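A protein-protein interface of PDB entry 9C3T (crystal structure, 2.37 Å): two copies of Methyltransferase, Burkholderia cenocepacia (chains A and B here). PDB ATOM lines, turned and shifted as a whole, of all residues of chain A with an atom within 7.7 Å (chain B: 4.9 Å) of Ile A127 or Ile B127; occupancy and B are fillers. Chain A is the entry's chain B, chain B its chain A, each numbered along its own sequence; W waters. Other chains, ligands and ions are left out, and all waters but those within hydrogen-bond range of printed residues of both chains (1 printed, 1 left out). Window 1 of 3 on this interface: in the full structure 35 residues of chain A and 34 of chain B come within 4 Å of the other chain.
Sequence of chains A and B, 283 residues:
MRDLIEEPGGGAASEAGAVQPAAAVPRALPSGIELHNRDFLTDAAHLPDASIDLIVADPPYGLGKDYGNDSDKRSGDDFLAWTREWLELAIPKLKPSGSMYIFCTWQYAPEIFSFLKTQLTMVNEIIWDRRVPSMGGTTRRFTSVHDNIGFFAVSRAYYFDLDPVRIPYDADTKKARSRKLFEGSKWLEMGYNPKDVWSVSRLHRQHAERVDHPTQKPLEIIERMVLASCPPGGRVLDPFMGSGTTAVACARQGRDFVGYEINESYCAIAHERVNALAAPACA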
ATOM      1  N   TRP A 106      -4.867   6.705 -16.742  1.00  0.00           N
ATOM      2  CA  TRP A 106      -3.975   7.739 -16.227  1.00  0.00           C
ATOM      3  C   TRP A 106      -3.381   8.594 -17.340  1.00  0.00           C
ATOM      4  O   TRP A 106      -2.996   9.742 -17.090  1.00  0.00           O
ATOM      5  CB  TRP A 106      -2.854   7.100 -15.404  1.00  0.00           C
ATOM      6  CG  TRP A 106      -2.015   6.135 -16.185  1.00  0.00           C
ATOM      7  CD1 TRP A 106      -2.255   4.805 -16.373  1.00  0.00           C
ATOM      8  CD2 TRP A 106      -0.803   6.427 -16.888  1.00  0.00           C
ATOM      9  NE1 TRP A 106      -1.266   4.250 -17.149  1.00  0.00           N
ATOM     10  CE2 TRP A 106      -0.362   5.225 -17.478  1.00  0.00           C
ATOM     11  CE3 TRP A 106      -0.046   7.587 -17.074  1.00  0.00           C
ATOM     12  CZ2 TRP A 106       0.801   5.152 -18.241  1.00  0.00           C
ATOM     13  CZ3 TRP A 106       1.108   7.512 -17.832  1.00  0.00           C
ATOM     14  CH2 TRP A 106       1.520   6.304 -18.406  1.00  0.00           C
ATOM     15  N   PHE A 113     -10.078  15.043 -15.693  1.00  0.00           N
ATOM     16  CA  PHE A 113     -10.527  15.487 -14.378  1.00  0.00           C
ATOM     17  C   PHE A 113     -10.384  16.993 -14.212  1.00  0.00           C
ATOM     18  O   PHE A 113     -11.170  17.610 -13.487  1.00  0.00           O
ATOM     19  CB  PHE A 113      -9.756  14.754 -13.279  1.00  0.00           C
ATOM     20  CG  PHE A 113     -10.083  13.290 -13.179  1.00  0.00           C
ATOM     21  CD1 PHE A 113     -11.112  12.741 -13.929  1.00  0.00           C
ATOM     22  CD2 PHE A 113      -9.361  12.464 -12.335  1.00  0.00           C
ATOM     23  CE1 PHE A 113     -11.413  11.397 -13.841  1.00  0.00           C
ATOM     24  CE2 PHE A 113      -9.657  11.116 -12.240  1.00  0.00           C
ATOM     25  CZ  PHE A 113     -10.684  10.582 -12.996  1.00  0.00           C
ATOM     26  N   ASN A 124     -14.483  12.487  -5.107  1.00  0.00           N
ATOM     27  CA  ASN A 124     -13.500  11.409  -4.866  1.00  0.00           C
ATOM     28  C   ASN A 124     -12.776  10.956  -6.129  1.00  0.00           C
ATOM     29  O   ASN A 124     -13.298  11.162  -7.229  1.00  0.00           O
ATOM     30  CB  ASN A 124     -14.152  10.167  -4.270  1.00  0.00           C
ATOM     31  CG  ASN A 124     -14.125  10.105  -2.766  1.00  0.00           C
ATOM     32  OD1 ASN A 124     -15.116   9.697  -2.157  1.00  0.00           O
ATOM     33  ND2 ASN A 124     -13.017  10.485  -2.153  1.00  0.00           N
ATOM     34  N   GLU A 125     -11.564  10.452  -5.962  1.00  0.00           N
ATOM     35  CA  GLU A 125     -10.848   9.776  -7.040  1.00  0.00           C
ATOM     36  C   GLU A 125     -10.719   8.321  -6.614  1.00  0.00           C
ATOM     37  O   GLU A 125      -9.884   7.983  -5.770  1.00  0.00           O
ATOM     38  CB  GLU A 125      -9.485  10.401  -7.317  1.00  0.00           C
ATOM     39  CG  GLU A 125      -8.798   9.789  -8.532  1.00  0.00           C
ATOM     40  CD  GLU A 125      -7.295   9.690  -8.380  1.00  0.00           C
ATOM     41  OE1 GLU A 125      -6.822   9.577  -7.230  1.00  0.00           O
ATOM     42  OE2 GLU A 125      -6.589   9.718  -9.412  1.00  0.00           O
ATOM     43  N   ILE A 126     -11.556   7.466  -7.183  1.00  0.00           N
ATOM     44  CA  ILE A 126     -11.562   6.048  -6.853  1.00  0.00           C
ATOM     45  C   ILE A 126     -10.579   5.332  -7.767  1.00  0.00           C
ATOM     46  O   ILE A 126     -10.641   5.470  -8.994  1.00  0.00           O
ATOM     47  CB  ILE A 126     -12.975   5.461  -6.986  1.00  0.00           C
ATOM     48  CG1 ILE A 126     -13.905   6.107  -5.959  1.00  0.00           C
ATOM     49  CG2 ILE A 126     -12.935   3.957  -6.792  1.00  0.00           C
ATOM     50  CD1 ILE A 126     -15.263   6.485  -6.501  1.00  0.00           C
ATOM     51  N   ILE A 127      -9.681   4.581  -7.151  1.00  0.00           N
ATOM     52  CA  ILE A 127      -8.678   3.808  -7.921  1.00  0.00           C
ATOM     53  C   ILE A 127      -9.144   2.348  -7.948  1.00  0.00           C
ATOM     54  O   ILE A 127      -9.257   1.754  -6.882  1.00  0.00           O
ATOM     55  CB  ILE A 127      -7.260   3.986  -7.336  1.00  0.00           C
ATOM     56  CG1 ILE A 127      -6.814   5.440  -7.378  1.00  0.00           C
ATOM     57  CG2 ILE A 127      -6.264   3.060  -8.033  1.00  0.00           C
ATOM     58  CD1 ILE A 127      -6.733   6.014  -8.779  1.00  0.00           C
ATOM     59  N   TRP A 128      -9.447   1.835  -9.133  1.00  0.00           N
ATOM     60  CA  TRP A 128      -9.793   0.402  -9.248  1.00  0.00           C
ATOM     61  C   TRP A 128      -8.530  -0.445  -9.409  1.00  0.00           C
ATOM     62  O   TRP A 128      -7.933  -0.436 -10.484  1.00  0.00           O
ATOM     63  CB  TRP A 128     -10.802   0.126 -10.371  1.00  0.00           C
ATOM     64  CG  TRP A 128     -11.013  -1.341 -10.628  1.00  0.00           C
ATOM     65  CD1 TRP A 128     -11.042  -2.340  -9.704  1.00  0.00           C
ATOM     66  CD2 TRP A 128     -11.206  -1.975 -11.907  1.00  0.00           C
ATOM     67  NE1 TRP A 128     -11.237  -3.546 -10.312  1.00  0.00           N
ATOM     68  CE2 TRP A 128     -11.347  -3.355 -11.661  1.00  0.00           C
ATOM     69  CE3 TRP A 128     -11.280  -1.513 -13.224  1.00  0.00           C
ATOM     70  CZ2 TRP A 128     -11.552  -4.275 -12.682  1.00  0.00           C
ATOM     71  CZ3 TRP A 128     -11.484  -2.425 -14.232  1.00  0.00           C
ATOM     72  CH2 TRP A 128     -11.616  -3.784 -13.963  1.00  0.00           C
ATOM     73  N   ASP A 129      -8.154  -1.141  -8.343  1.00  0.00           N
ATOM     74  CA  ASP A 129      -7.033  -2.105  -8.422  1.00  0.00           C
ATOM     75  C   ASP A 129      -7.560  -3.383  -9.075  1.00  0.00           C
ATOM     76  O   ASP A 129      -8.212  -4.170  -8.390  1.00  0.00           O
ATOM     77  CB  ASP A 129      -6.388  -2.319  -7.069  1.00  0.00           C
ATOM     78  CG  ASP A 129      -5.187  -3.253  -7.040  1.00  0.00           C
ATOM     79  OD1 ASP A 129      -4.650  -3.562  -8.122  1.00  0.00           O
ATOM     80  OD2 ASP A 129      -4.799  -3.659  -5.932  1.00  0.00           O
ATOM     81  N   ARG A 130      -7.234  -3.577 -10.345  1.00  0.00           N
ATOM     82  CA  ARG A 130      -7.705  -4.744 -11.122  1.00  0.00           C
ATOM     83  C   ARG A 130      -6.907  -5.995 -10.742  1.00  0.00           C
ATOM     84  O   ARG A 130      -7.162  -7.021 -11.368  1.00  0.00           O
ATOM     85  CB  ARG A 130      -7.644  -4.313 -12.589  1.00  0.00           C
ATOM     86  CG  ARG A 130      -7.762  -2.835 -12.922  1.00  0.00           C
ATOM     87  CD  ARG A 130      -7.614  -2.624 -14.418  1.00  0.00           C
ATOM     88  NE  ARG A 130      -6.380  -3.165 -14.995  1.00  0.00           N
ATOM     89  CZ  ARG A 130      -5.463  -2.444 -15.622  1.00  0.00           C
ATOM     90  NH1 ARG A 130      -5.559  -1.133 -15.641  1.00  0.00           N
ATOM     91  NH2 ARG A 130      -4.449  -3.029 -16.225  1.00  0.00           N
ATOM     92  N   VAL A 145      -2.066  -1.712 -13.497  1.00  0.00           N
ATOM     93  CA  VAL A 145      -2.919  -2.628 -12.691  1.00  0.00           C
ATOM     94  C   VAL A 145      -4.087  -1.787 -12.160  1.00  0.00           C
ATOM     95  O   VAL A 145      -4.866  -2.278 -11.329  1.00  0.00           O
ATOM     96  CB  VAL A 145      -2.130  -3.319 -11.562  1.00  0.00           C
ATOM     97  CG1 VAL A 145      -1.862  -2.408 -10.374  1.00  0.00           C
ATOM     98  CG2 VAL A 145      -2.761  -4.633 -11.129  1.00  0.00           C
ATOM     99  N   HIS A 146      -4.209  -0.558 -12.648  1.00  0.00           N
ATOM    100  CA  HIS A 146      -5.274   0.327 -12.115  1.00  0.00           C
ATOM    101  C   HIS A 146      -5.942   1.230 -13.143  1.00  0.00           C
ATOM    102  O   HIS A 146      -5.284   1.682 -14.064  1.00  0.00           O
ATOM    103  CB  HIS A 146      -4.741   1.204 -10.978  1.00  0.00           C
ATOM    104  CG  HIS A 146      -4.201   2.546 -11.333  1.00  0.00           C
ATOM    105  ND1 HIS A 146      -2.915   2.730 -11.783  1.00  0.00           N
ATOM    106  CD2 HIS A 146      -4.747   3.761 -11.278  1.00  0.00           C
ATOM    107  CE1 HIS A 146      -2.710   4.015 -12.005  1.00  0.00           C
ATOM    108  NE2 HIS A 146      -3.808   4.658 -11.705  1.00  0.00           N
ATOM    109  N   ASP A 147      -7.244   1.411 -13.003  1.00  0.00           N
ATOM    110  CA  ASP A 147      -7.969   2.415 -13.765  1.00  0.00           C
ATOM    111  C   ASP A 147      -8.430   3.520 -12.824  1.00  0.00           C
ATOM    112  O   ASP A 147      -8.608   3.308 -11.623  1.00  0.00           O
ATOM    113  CB  ASP A 147      -9.178   1.808 -14.489  1.00  0.00           C
ATOM    114  CG  ASP A 147      -8.792   0.705 -15.458  1.00  0.00           C
ATOM    115  OD1 ASP A 147      -7.580   0.480 -15.659  1.00  0.00           O
ATOM    116  OD2 ASP A 147      -9.703   0.063 -16.022  1.00  0.00           O
ATOM    117  N   ASN A 148      -8.624   4.711 -13.382  1.00  0.00           N
ATOM    118  CA  ASN A 148      -9.030   5.877 -12.611  1.00  0.00           C
ATOM    119  C   ASN A 148     -10.523   6.119 -12.793  1.00  0.00           C
ATOM    120  O   ASN A 148     -11.013   6.172 -13.926  1.00  0.00           O
ATOM    121  CB  ASN A 148      -8.238   7.114 -13.038  1.00  0.00           C
ATOM    122  CG  ASN A 148      -6.742   6.928 -12.878  1.00  0.00           C
ATOM    123  OD1 ASN A 148      -6.131   6.112 -13.569  1.00  0.00           O
ATOM    124  ND2 ASN A 148      -6.146   7.680 -11.960  1.00  0.00           N
ATOM    125  N   ILE A 149     -11.238   6.262 -11.679  1.00  0.00           N
ATOM    126  CA  ILE A 149     -12.660   6.586 -11.687  1.00  0.00           C
ATOM    127  C   ILE A 149     -12.837   7.937 -11.007  1.00  0.00           C
ATOM    128  O   ILE A 149     -12.451   8.108  -9.844  1.00  0.00           O
ATOM    129  CB  ILE A 149     -13.506   5.511 -10.987  1.00  0.00           C
ATOM    130  CG1 ILE A 149     -13.253   4.132 -11.603  1.00  0.00           C
ATOM    131  CG2 ILE A 149     -14.981   5.877 -11.063  1.00  0.00           C
ATOM    132  CD1 ILE A 149     -13.466   2.973 -10.639  1.00  0.00           C
ATOM    133  N   GLY A 150     -13.482   8.856 -11.700  1.00  0.00           N
ATOM    134  CA  GLY A 150     -13.782  10.167 -11.111  1.00  0.00           C
ATOM    135  C   GLY A 150     -15.180  10.223 -10.545  1.00  0.00           C
ATOM    136  O   GLY A 150     -16.112   9.846 -11.257  1.00  0.00           O
ATOM    137  N   LYS A 195     -13.690   2.631   0.755  1.00  0.00           N
ATOM    138  CA  LYS A 195     -12.482   3.485   0.524  1.00  0.00           C
ATOM    139  C   LYS A 195     -12.367   3.940  -0.949  1.00  0.00           C
ATOM    140  O   LYS A 195     -13.256   3.600  -1.728  1.00  0.00           O
ATOM    141  CB  LYS A 195     -11.226   2.830   1.116  1.00  0.00           C
ATOM    142  CG  LYS A 195     -11.337   2.267   2.519  1.00  0.00           C
ATOM    143  CD  LYS A 195     -10.006   2.176   3.249  1.00  0.00           C
ATOM    144  CE  LYS A 195      -9.664   0.793   3.683  1.00  0.00           C
ATOM    145  NZ  LYS A 195     -10.627   0.263   4.645  1.00  0.00           N
ATOM    146  N   ASP A 196     -11.318   4.687  -1.290  1.00  0.00           N
ATOM    147  CA  ASP A 196     -11.092   5.214  -2.667  1.00  0.00           C
ATOM    148  C   ASP A 196     -10.185   4.273  -3.469  1.00  0.00           C
ATOM    149  O   ASP A 196      -9.720   4.684  -4.527  1.00  0.00           O
ATOM    150  CB  ASP A 196     -10.583   6.646  -2.620  1.00  0.00           C
ATOM    151  CG  ASP A 196      -9.261   6.896  -1.916  1.00  0.00           C
ATOM    152  OD1 ASP A 196      -8.689   5.940  -1.375  1.00  0.00           O
ATOM    153  OD2 ASP A 196      -8.820   8.052  -1.927  1.00  0.00           O
ATOM    154  N   VAL A 197      -9.879   3.106  -2.923  1.00  0.00           N
ATOM    155  CA  VAL A 197      -9.148   2.107  -3.696  1.00  0.00           C
ATOM    156  C   VAL A 197      -9.924   0.805  -3.596  1.00  0.00           C
ATOM    157  O   VAL A 197     -10.158   0.301  -2.491  1.00  0.00           O
ATOM    158  CB  VAL A 197      -7.702   1.916  -3.210  1.00  0.00           C
ATOM    159  CG1 VAL A 197      -7.047   0.755  -3.950  1.00  0.00           C
ATOM    160  CG2 VAL A 197      -6.910   3.179  -3.432  1.00  0.00           C
ATOM    161  N   TRP A 198     -10.342   0.325  -4.755  1.00  0.00           N
ATOM    162  CA  TRP A 198     -11.166  -0.893  -4.811  1.00  0.00           C
ATOM    163  C   TRP A 198     -10.367  -2.039  -5.430  1.00  0.00           C
ATOM    164  O   TRP A 198     -10.182  -2.049  -6.644  1.00  0.00           O
ATOM    165  CB  TRP A 198     -12.459  -0.590  -5.574  1.00  0.00           C
ATOM    166  CG  TRP A 198     -13.316   0.499  -4.988  1.00  0.00           C
ATOM    167  CD1 TRP A 198     -13.202   1.086  -3.765  1.00  0.00           C
ATOM    168  CD2 TRP A 198     -14.452   1.119  -5.624  1.00  0.00           C
ATOM    169  NE1 TRP A 198     -14.173   2.032  -3.599  1.00  0.00           N
ATOM    170  CE2 TRP A 198     -14.956   2.075  -4.719  1.00  0.00           C
ATOM    171  CE3 TRP A 198     -15.081   0.965  -6.861  1.00  0.00           C
ATOM    172  CZ2 TRP A 198     -16.057   2.871  -5.016  1.00  0.00           C
ATOM    173  CZ3 TRP A 198     -16.173   1.750  -7.151  1.00  0.00           C
ATOM    174  CH2 TRP A 198     -16.651   2.690  -6.242  1.00  0.00           C
ATOM    175  N   SER A 199      -9.938  -2.975  -4.593  1.00  0.00           N
ATOM    176  CA  SER A 199      -9.169  -4.152  -5.062  1.00  0.00           C
ATOM    177  C   SER A 199     -10.120  -5.266  -5.510  1.00  0.00           C
ATOM    178  O   SER A 199     -10.331  -6.207  -4.754  1.00  0.00           O
ATOM    179  CB  SER A 199      -8.197  -4.622  -4.032  1.00  0.00           C
ATOM    180  OG  SER A 199      -6.886  -4.161  -4.308  1.00  0.00           O
ATOM    181  N   VAL A 200     -10.675  -5.119  -6.697  1.00  0.00           N
ATOM    182  CA  VAL A 200     -11.564  -6.152  -7.285  1.00  0.00           C
ATOM    183  C   VAL A 200     -10.869  -6.672  -8.548  1.00  0.00           C
ATOM    184  O   VAL A 200     -10.491  -5.858  -9.388  1.00  0.00           O
ATOM    185  CB  VAL A 200     -12.974  -5.588  -7.549  1.00  0.00           C
ATOM    186  CG1 VAL A 200     -13.916  -6.643  -8.106  1.00  0.00           C
ATOM    187  CG2 VAL A 200     -13.555  -4.933  -6.306  1.00  0.00           C
ATOM    188  N   ILE A 221     -18.220  -3.485  -8.668  1.00  0.00           N
ATOM    189  CA  ILE A 221     -17.872  -2.041  -8.543  1.00  0.00           C
ATOM    190  C   ILE A 221     -18.984  -1.160  -9.137  1.00  0.00           C
ATOM    191  O   ILE A 221     -19.195  -0.064  -8.607  1.00  0.00           O
ATOM    192  CB  ILE A 221     -16.475  -1.775  -9.140  1.00  0.00           C
ATOM    193  CG1 ILE A 221     -16.412  -2.052 -10.639  1.00  0.00           C
ATOM    194  CG2 ILE A 221     -15.408  -2.558  -8.380  1.00  0.00           C
ATOM    195  CD1 ILE A 221     -15.055  -1.782 -11.260  1.00  0.00           C
ATOM    196  N   GLU B 125       1.645   6.655 -13.561  1.00  0.00           N
ATOM    197  CA  GLU B 125       0.948   7.146 -12.379  1.00  0.00           C
ATOM    198  C   GLU B 125       0.961   6.011 -11.367  1.00  0.00           C
ATOM    199  O   GLU B 125       0.294   4.989 -11.566  1.00  0.00           O
ATOM    200  CB  GLU B 125      -0.482   7.586 -12.682  1.00  0.00           C
ATOM    201  CG  GLU B 125      -1.087   8.393 -11.539  1.00  0.00           C
ATOM    202  CD  GLU B 125      -2.601   8.371 -11.518  1.00  0.00           C
ATOM    203  OE1 GLU B 125      -3.188   7.350 -11.931  1.00  0.00           O
ATOM    204  OE2 GLU B 125      -3.204   9.375 -11.078  1.00  0.00           O
ATOM    205  N   ILE B 126       1.733   6.180 -10.300  1.00  0.00           N
ATOM    206  CA  ILE B 126       1.859   5.177  -9.251  1.00  0.00           C
ATOM    207  C   ILE B 126       0.906   5.538  -8.121  1.00  0.00           C
ATOM    208  O   ILE B 126       0.920   6.670  -7.621  1.00  0.00           O
ATOM    209  CB  ILE B 126       3.307   5.076  -8.747  1.00  0.00           C
ATOM    210  CG1 ILE B 126       4.189   4.439  -9.823  1.00  0.00           C
ATOM    211  CG2 ILE B 126       3.370   4.273  -7.459  1.00  0.00           C
ATOM    212  CD1 ILE B 126       5.507   5.146 -10.038  1.00  0.00           C
ATOM    213  N   ILE B 127       0.087   4.570  -7.739  1.00  0.00           N
ATOM    214  CA  ILE B 127      -0.881   4.778  -6.632  1.00  0.00           C
ATOM    215  C   ILE B 127      -0.321   4.127  -5.367  1.00  0.00           C
ATOM    216  O   ILE B 127      -0.189   2.908  -5.340  1.00  0.00           O
ATOM    217  CB  ILE B 127      -2.280   4.252  -7.005  1.00  0.00           C
ATOM    218  CG1 ILE B 127      -2.764   4.841  -8.326  1.00  0.00           C
ATOM    219  CG2 ILE B 127      -3.281   4.492  -5.878  1.00  0.00           C
ATOM    220  CD1 ILE B 127      -2.965   6.343  -8.297  1.00  0.00           C
ATOM    221  N   TRP B 128       0.035   4.940  -4.386  1.00  0.00           N
ATOM    222  CA  TRP B 128       0.461   4.385  -3.087  1.00  0.00           C
ATOM    223  C   TRP B 128      -0.775   4.055  -2.243  1.00  0.00           C
ATOM    224  O   TRP B 128      -1.438   4.985  -1.773  1.00  0.00           O
ATOM    225  CB  TRP B 128       1.422   5.323  -2.350  1.00  0.00           C
ATOM    226  CG  TRP B 128       1.736   4.856  -0.955  1.00  0.00           C
ATOM    227  CD1 TRP B 128       1.898   3.569  -0.536  1.00  0.00           C
ATOM    228  CD2 TRP B 128       1.904   5.679   0.216  1.00  0.00           C
ATOM    229  NE1 TRP B 128       2.157   3.531   0.805  1.00  0.00           N
ATOM    230  CE2 TRP B 128       2.170   4.808   1.293  1.00  0.00           C
ATOM    231  CE3 TRP B 128       1.861   7.053   0.455  1.00  0.00           C
ATOM    232  CZ2 TRP B 128       2.385   5.273   2.586  1.00  0.00           C
ATOM    233  CZ3 TRP B 128       2.076   7.509   1.734  1.00  0.00           C
ATOM    234  CH2 TRP B 128       2.333   6.631   2.782  1.00  0.00           C
ATOM    235  N   ASP B 129      -1.074   2.764  -2.106  1.00  0.00           N
ATOM    236  CA  ASP B 129      -2.176   2.318  -1.226  1.00  0.00           C
ATOM    237  C   ASP B 129      -1.615   2.258   0.188  1.00  0.00           C
ATOM    238  O   ASP B 129      -0.802   1.375   0.455  1.00  0.00           O
ATOM    239  CB  ASP B 129      -2.797   1.025  -1.710  1.00  0.00           C
ATOM    240  CG  ASP B 129      -3.864   0.409  -0.817  1.00  0.00           C
ATOM    241  OD1 ASP B 129      -4.420   1.130   0.027  1.00  0.00           O
ATOM    242  OD2 ASP B 129      -4.133  -0.788  -0.989  1.00  0.00           O
ATOM    243  N   HIS B 146      -5.366   6.439  -0.519  1.00  0.00           N
ATOM    244  CA  HIS B 146      -4.317   6.489  -1.565  1.00  0.00           C
ATOM    245  C   HIS B 146      -3.691   7.856  -1.817  1.00  0.00           C
ATOM    246  O   HIS B 146      -4.386   8.877  -1.785  1.00  0.00           O
ATOM    247  CB  HIS B 146      -4.824   5.945  -2.905  1.00  0.00           C
ATOM    248  CG  HIS B 146      -5.457   6.905  -3.835  1.00  0.00           C
ATOM    249  ND1 HIS B 146      -6.810   7.129  -3.822  1.00  0.00           N
ATOM    250  CD2 HIS B 146      -4.964   7.656  -4.812  1.00  0.00           C
ATOM    251  CE1 HIS B 146      -7.106   8.018  -4.744  1.00  0.00           C
ATOM    252  NE2 HIS B 146      -6.002   8.346  -5.359  1.00  0.00           N
ATOM    253  N   ASP B 147      -2.382   7.866  -2.025  1.00  0.00           N
ATOM    254  CA  ASP B 147      -1.713   9.060  -2.509  1.00  0.00           C
ATOM    255  C   ASP B 147      -1.332   8.860  -3.970  1.00  0.00           C
ATOM    256  O   ASP B 147      -1.132   7.730  -4.427  1.00  0.00           O
ATOM    257  CB  ASP B 147      -0.459   9.374  -1.683  1.00  0.00           C
ATOM    258  CG  ASP B 147      -0.786   9.901  -0.298  1.00  0.00           C
ATOM    259  OD1 ASP B 147      -1.982  10.107  -0.005  1.00  0.00           O
ATOM    260  OD2 ASP B 147       0.158  10.114   0.492  1.00  0.00           O
ATOM    261  N   ASN B 148      -1.235   9.965  -4.702  1.00  0.00           N
ATOM    262  CA  ASN B 148      -0.903   9.939  -6.118  1.00  0.00           C
ATOM    263  C   ASN B 148       0.579  10.240  -6.303  1.00  0.00           C
ATOM    264  O   ASN B 148       1.086  11.227  -5.762  1.00  0.00           O
ATOM    265  CB  ASN B 148      -1.749  10.952  -6.893  1.00  0.00           C
ATOM    266  CG  ASN B 148      -3.212  10.559  -6.959  1.00  0.00           C
ATOM    267  OD1 ASN B 148      -3.947  10.697  -5.981  1.00  0.00           O
ATOM    268  ND2 ASN B 148      -3.642  10.066  -8.116  1.00  0.00           N
ATOM    269  N   ASP B 196       1.788  -0.327 -10.924  1.00  0.00           N
ATOM    270  CA  ASP B 196       1.543   1.116 -10.660  1.00  0.00           C
ATOM    271  C   ASP B 196       0.676   1.283  -9.414  1.00  0.00           C
ATOM    272  O   ASP B 196       0.204   2.391  -9.170  1.00  0.00           O
ATOM    273  CB  ASP B 196       0.980   1.796 -11.892  1.00  0.00           C
ATOM    274  CG  ASP B 196      -0.236   1.168 -12.540  1.00  0.00           C
ATOM    275  OD1 ASP B 196      -0.819   0.249 -11.944  1.00  0.00           O
ATOM    276  OD2 ASP B 196      -0.583   1.627 -13.631  1.00  0.00           O
ATOM    277  N   VAL B 197       0.413   0.195  -8.708  1.00  0.00           N
ATOM    278  CA  VAL B 197      -0.298   0.317  -7.412  1.00  0.00           C
ATOM    279  C   VAL B 197       0.625  -0.351  -6.382  1.00  0.00           C
ATOM    280  O   VAL B 197       0.868  -1.549  -6.506  1.00  0.00           O
ATOM    281  CB  VAL B 197      -1.750  -0.200  -7.296  1.00  0.00           C
ATOM    282  CG1 VAL B 197      -2.264  -0.117  -5.866  1.00  0.00           C
ATOM    283  CG2 VAL B 197      -2.690   0.540  -8.232  1.00  0.00           C
ATOM    284  N   TRP B 198       1.124   0.435  -5.438  1.00  0.00           N
ATOM    285  CA  TRP B 198       2.030  -0.080  -4.389  1.00  0.00           C
ATOM    286  C   TRP B 198       1.284  -0.141  -3.053  1.00  0.00           C
ATOM    287  O   TRP B 198       1.045   0.905  -2.446  1.00  0.00           O
ATOM    288  CB  TRP B 198       3.297   0.781  -4.306  1.00  0.00           C
ATOM    289  CG  TRP B 198       4.081   0.934  -5.580  1.00  0.00           C
ATOM    290  CD1 TRP B 198       3.913   0.271  -6.758  1.00  0.00           C
ATOM    291  CD2 TRP B 198       5.186   1.837  -5.787  1.00  0.00           C
ATOM    292  NE1 TRP B 198       4.824   0.702  -7.681  1.00  0.00           N
ATOM    293  CE2 TRP B 198       5.620   1.659  -7.115  1.00  0.00           C
ATOM    294  CE3 TRP B 198       5.842   2.774  -4.984  1.00  0.00           C
ATOM    295  CZ2 TRP B 198       6.676   2.386  -7.656  1.00  0.00           C
ATOM    296  CZ3 TRP B 198       6.888   3.490  -5.519  1.00  0.00           C
ATOM    297  CH2 TRP B 198       7.296   3.299  -6.836  1.00  0.00           C
HETATM  298  O   HOH W   1       0.786   4.074 -14.739  1.00  0.00           O
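A ring nitrogen (NE2) of His B146 sits close to the side-chain carboxylate of Glu A125, 2.4 Å away. The side-chain carboxylate (OD1) of Asp B196 is in hydrogen-bond range of the backbone NH (N) of Val A145 (2.8 Å). NE2 of His A146 is in hydrogen-bond range of OE1 of Glu B125 (2.8 Å). OD2 of Asp B196 sits at hydrogen-bond distance from ND1 of His A146, at 3.2 Å. The side-chain amide nitrogen (ND2) of Asn B148 sits at hydrogen-bond distance from the side-chain carboxylate (OE2) of Glu A125 (3.2 Å). The side-chain carboxylate (OE1) of Glu B125 is in hydrogen-bond range of the side-chain amide nitrogen (ND2) of Asn A148 (3.0 Å). The side-chain carboxylate (OD2) of Asp A196 sits at hydrogen-bond distance from a ring nitrogen (ND1) of His B146, 2.9 Å away.
OD1 of Asn A148 is in hydrogen-bond range of NE2 of His A146 (3.3 Å). The backbone NH of Ile B127 lies within hydrogen-bond range of the backbone carbonyl oxygen of Asp B196 (2.6 Å). The backbone NH (N) of Ile A127 sits at hydrogen-bond distance from the backbone carbonyl oxygen (O) of Asp A196. OE2 of Glu A125 sits at hydrogen-bond distance from ND2 of Asn A148 (3.3 Å). OD1 of Asn B148 lies within hydrogen-bond range of NE2 of His B146 (3.2 Å). O of His A146 is in hydrogen-bond range of NH1 of Arg A130 (3.2 Å).
Among the printed residues, merely in contact across the chains: Trp A106 with Glu B125 (3.5 Å), Glu A125 with Glu B125 (3.8 Å), Ile A127 with Ile B127 (3.8 Å), Ile A127 with His B146 (3.6 Å), Val A145 with Val B197 (3.7 Å), His A146 with Ile B127 (3.5 Å), His A146 with Val B197 (3.5 Å) and Val A197 with His B146 (3.5 Å).
Of the printed residues of chain B, Ile A127 touches Ile B127 and His B146. Ile B127 touches just these residues of chain A: Ile A127 (3.8 Å) and His A146 (3.5 Å). Printed residues of chain A within 4 Å of His B146: Glu A125, Ile A127, Asp A196 and Val A197. Of the printed residues of chain A, Asn B148 touches Glu A125. Of the printed residues of chain B, Asn A148 touches Glu B125 (3.0 Å). Of the printed residues of chain B, Val A197 touches His B146 (3.5 Å). Trp B128 touches none of the printed residues of chain A. Val A200 touches none of the printed residues of chain B. The nearest printed residue of chain B that does not touch His A146 is Ile B126 (5.2 Å).
Printed residues of chain B that touch a printed residue of chain A: Glu B125, Ile B127, His B146, Asn B148, Asp B196 and Val B197. Hydrophobic or aromatic side chains of chain B within 4 Å of the printed part of chain A: Ile B127, His B146 and Val B197. Hydrophobic or aromatic side chains of chain A that line the printed part of chain B: Trp A106, Ile A127, Val A145, His A146 and Val A197.
Glu A125 touches its own counterpart, Glu B125. Glu A125 touches His B146, and with the chains exchanged His A146 touches Glu B125. Ile A127 touches its own counterpart, Ile B127. His A146 touches Val B197, and with the chains exchanged Val A197 touches His B146.
Water W1 lies within hydrogen-bond range of N of Glu B125 (3.0 Å), OD2 of Asp B196 (3.0 Å) and NE1 of Trp A106 (3.2 Å).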
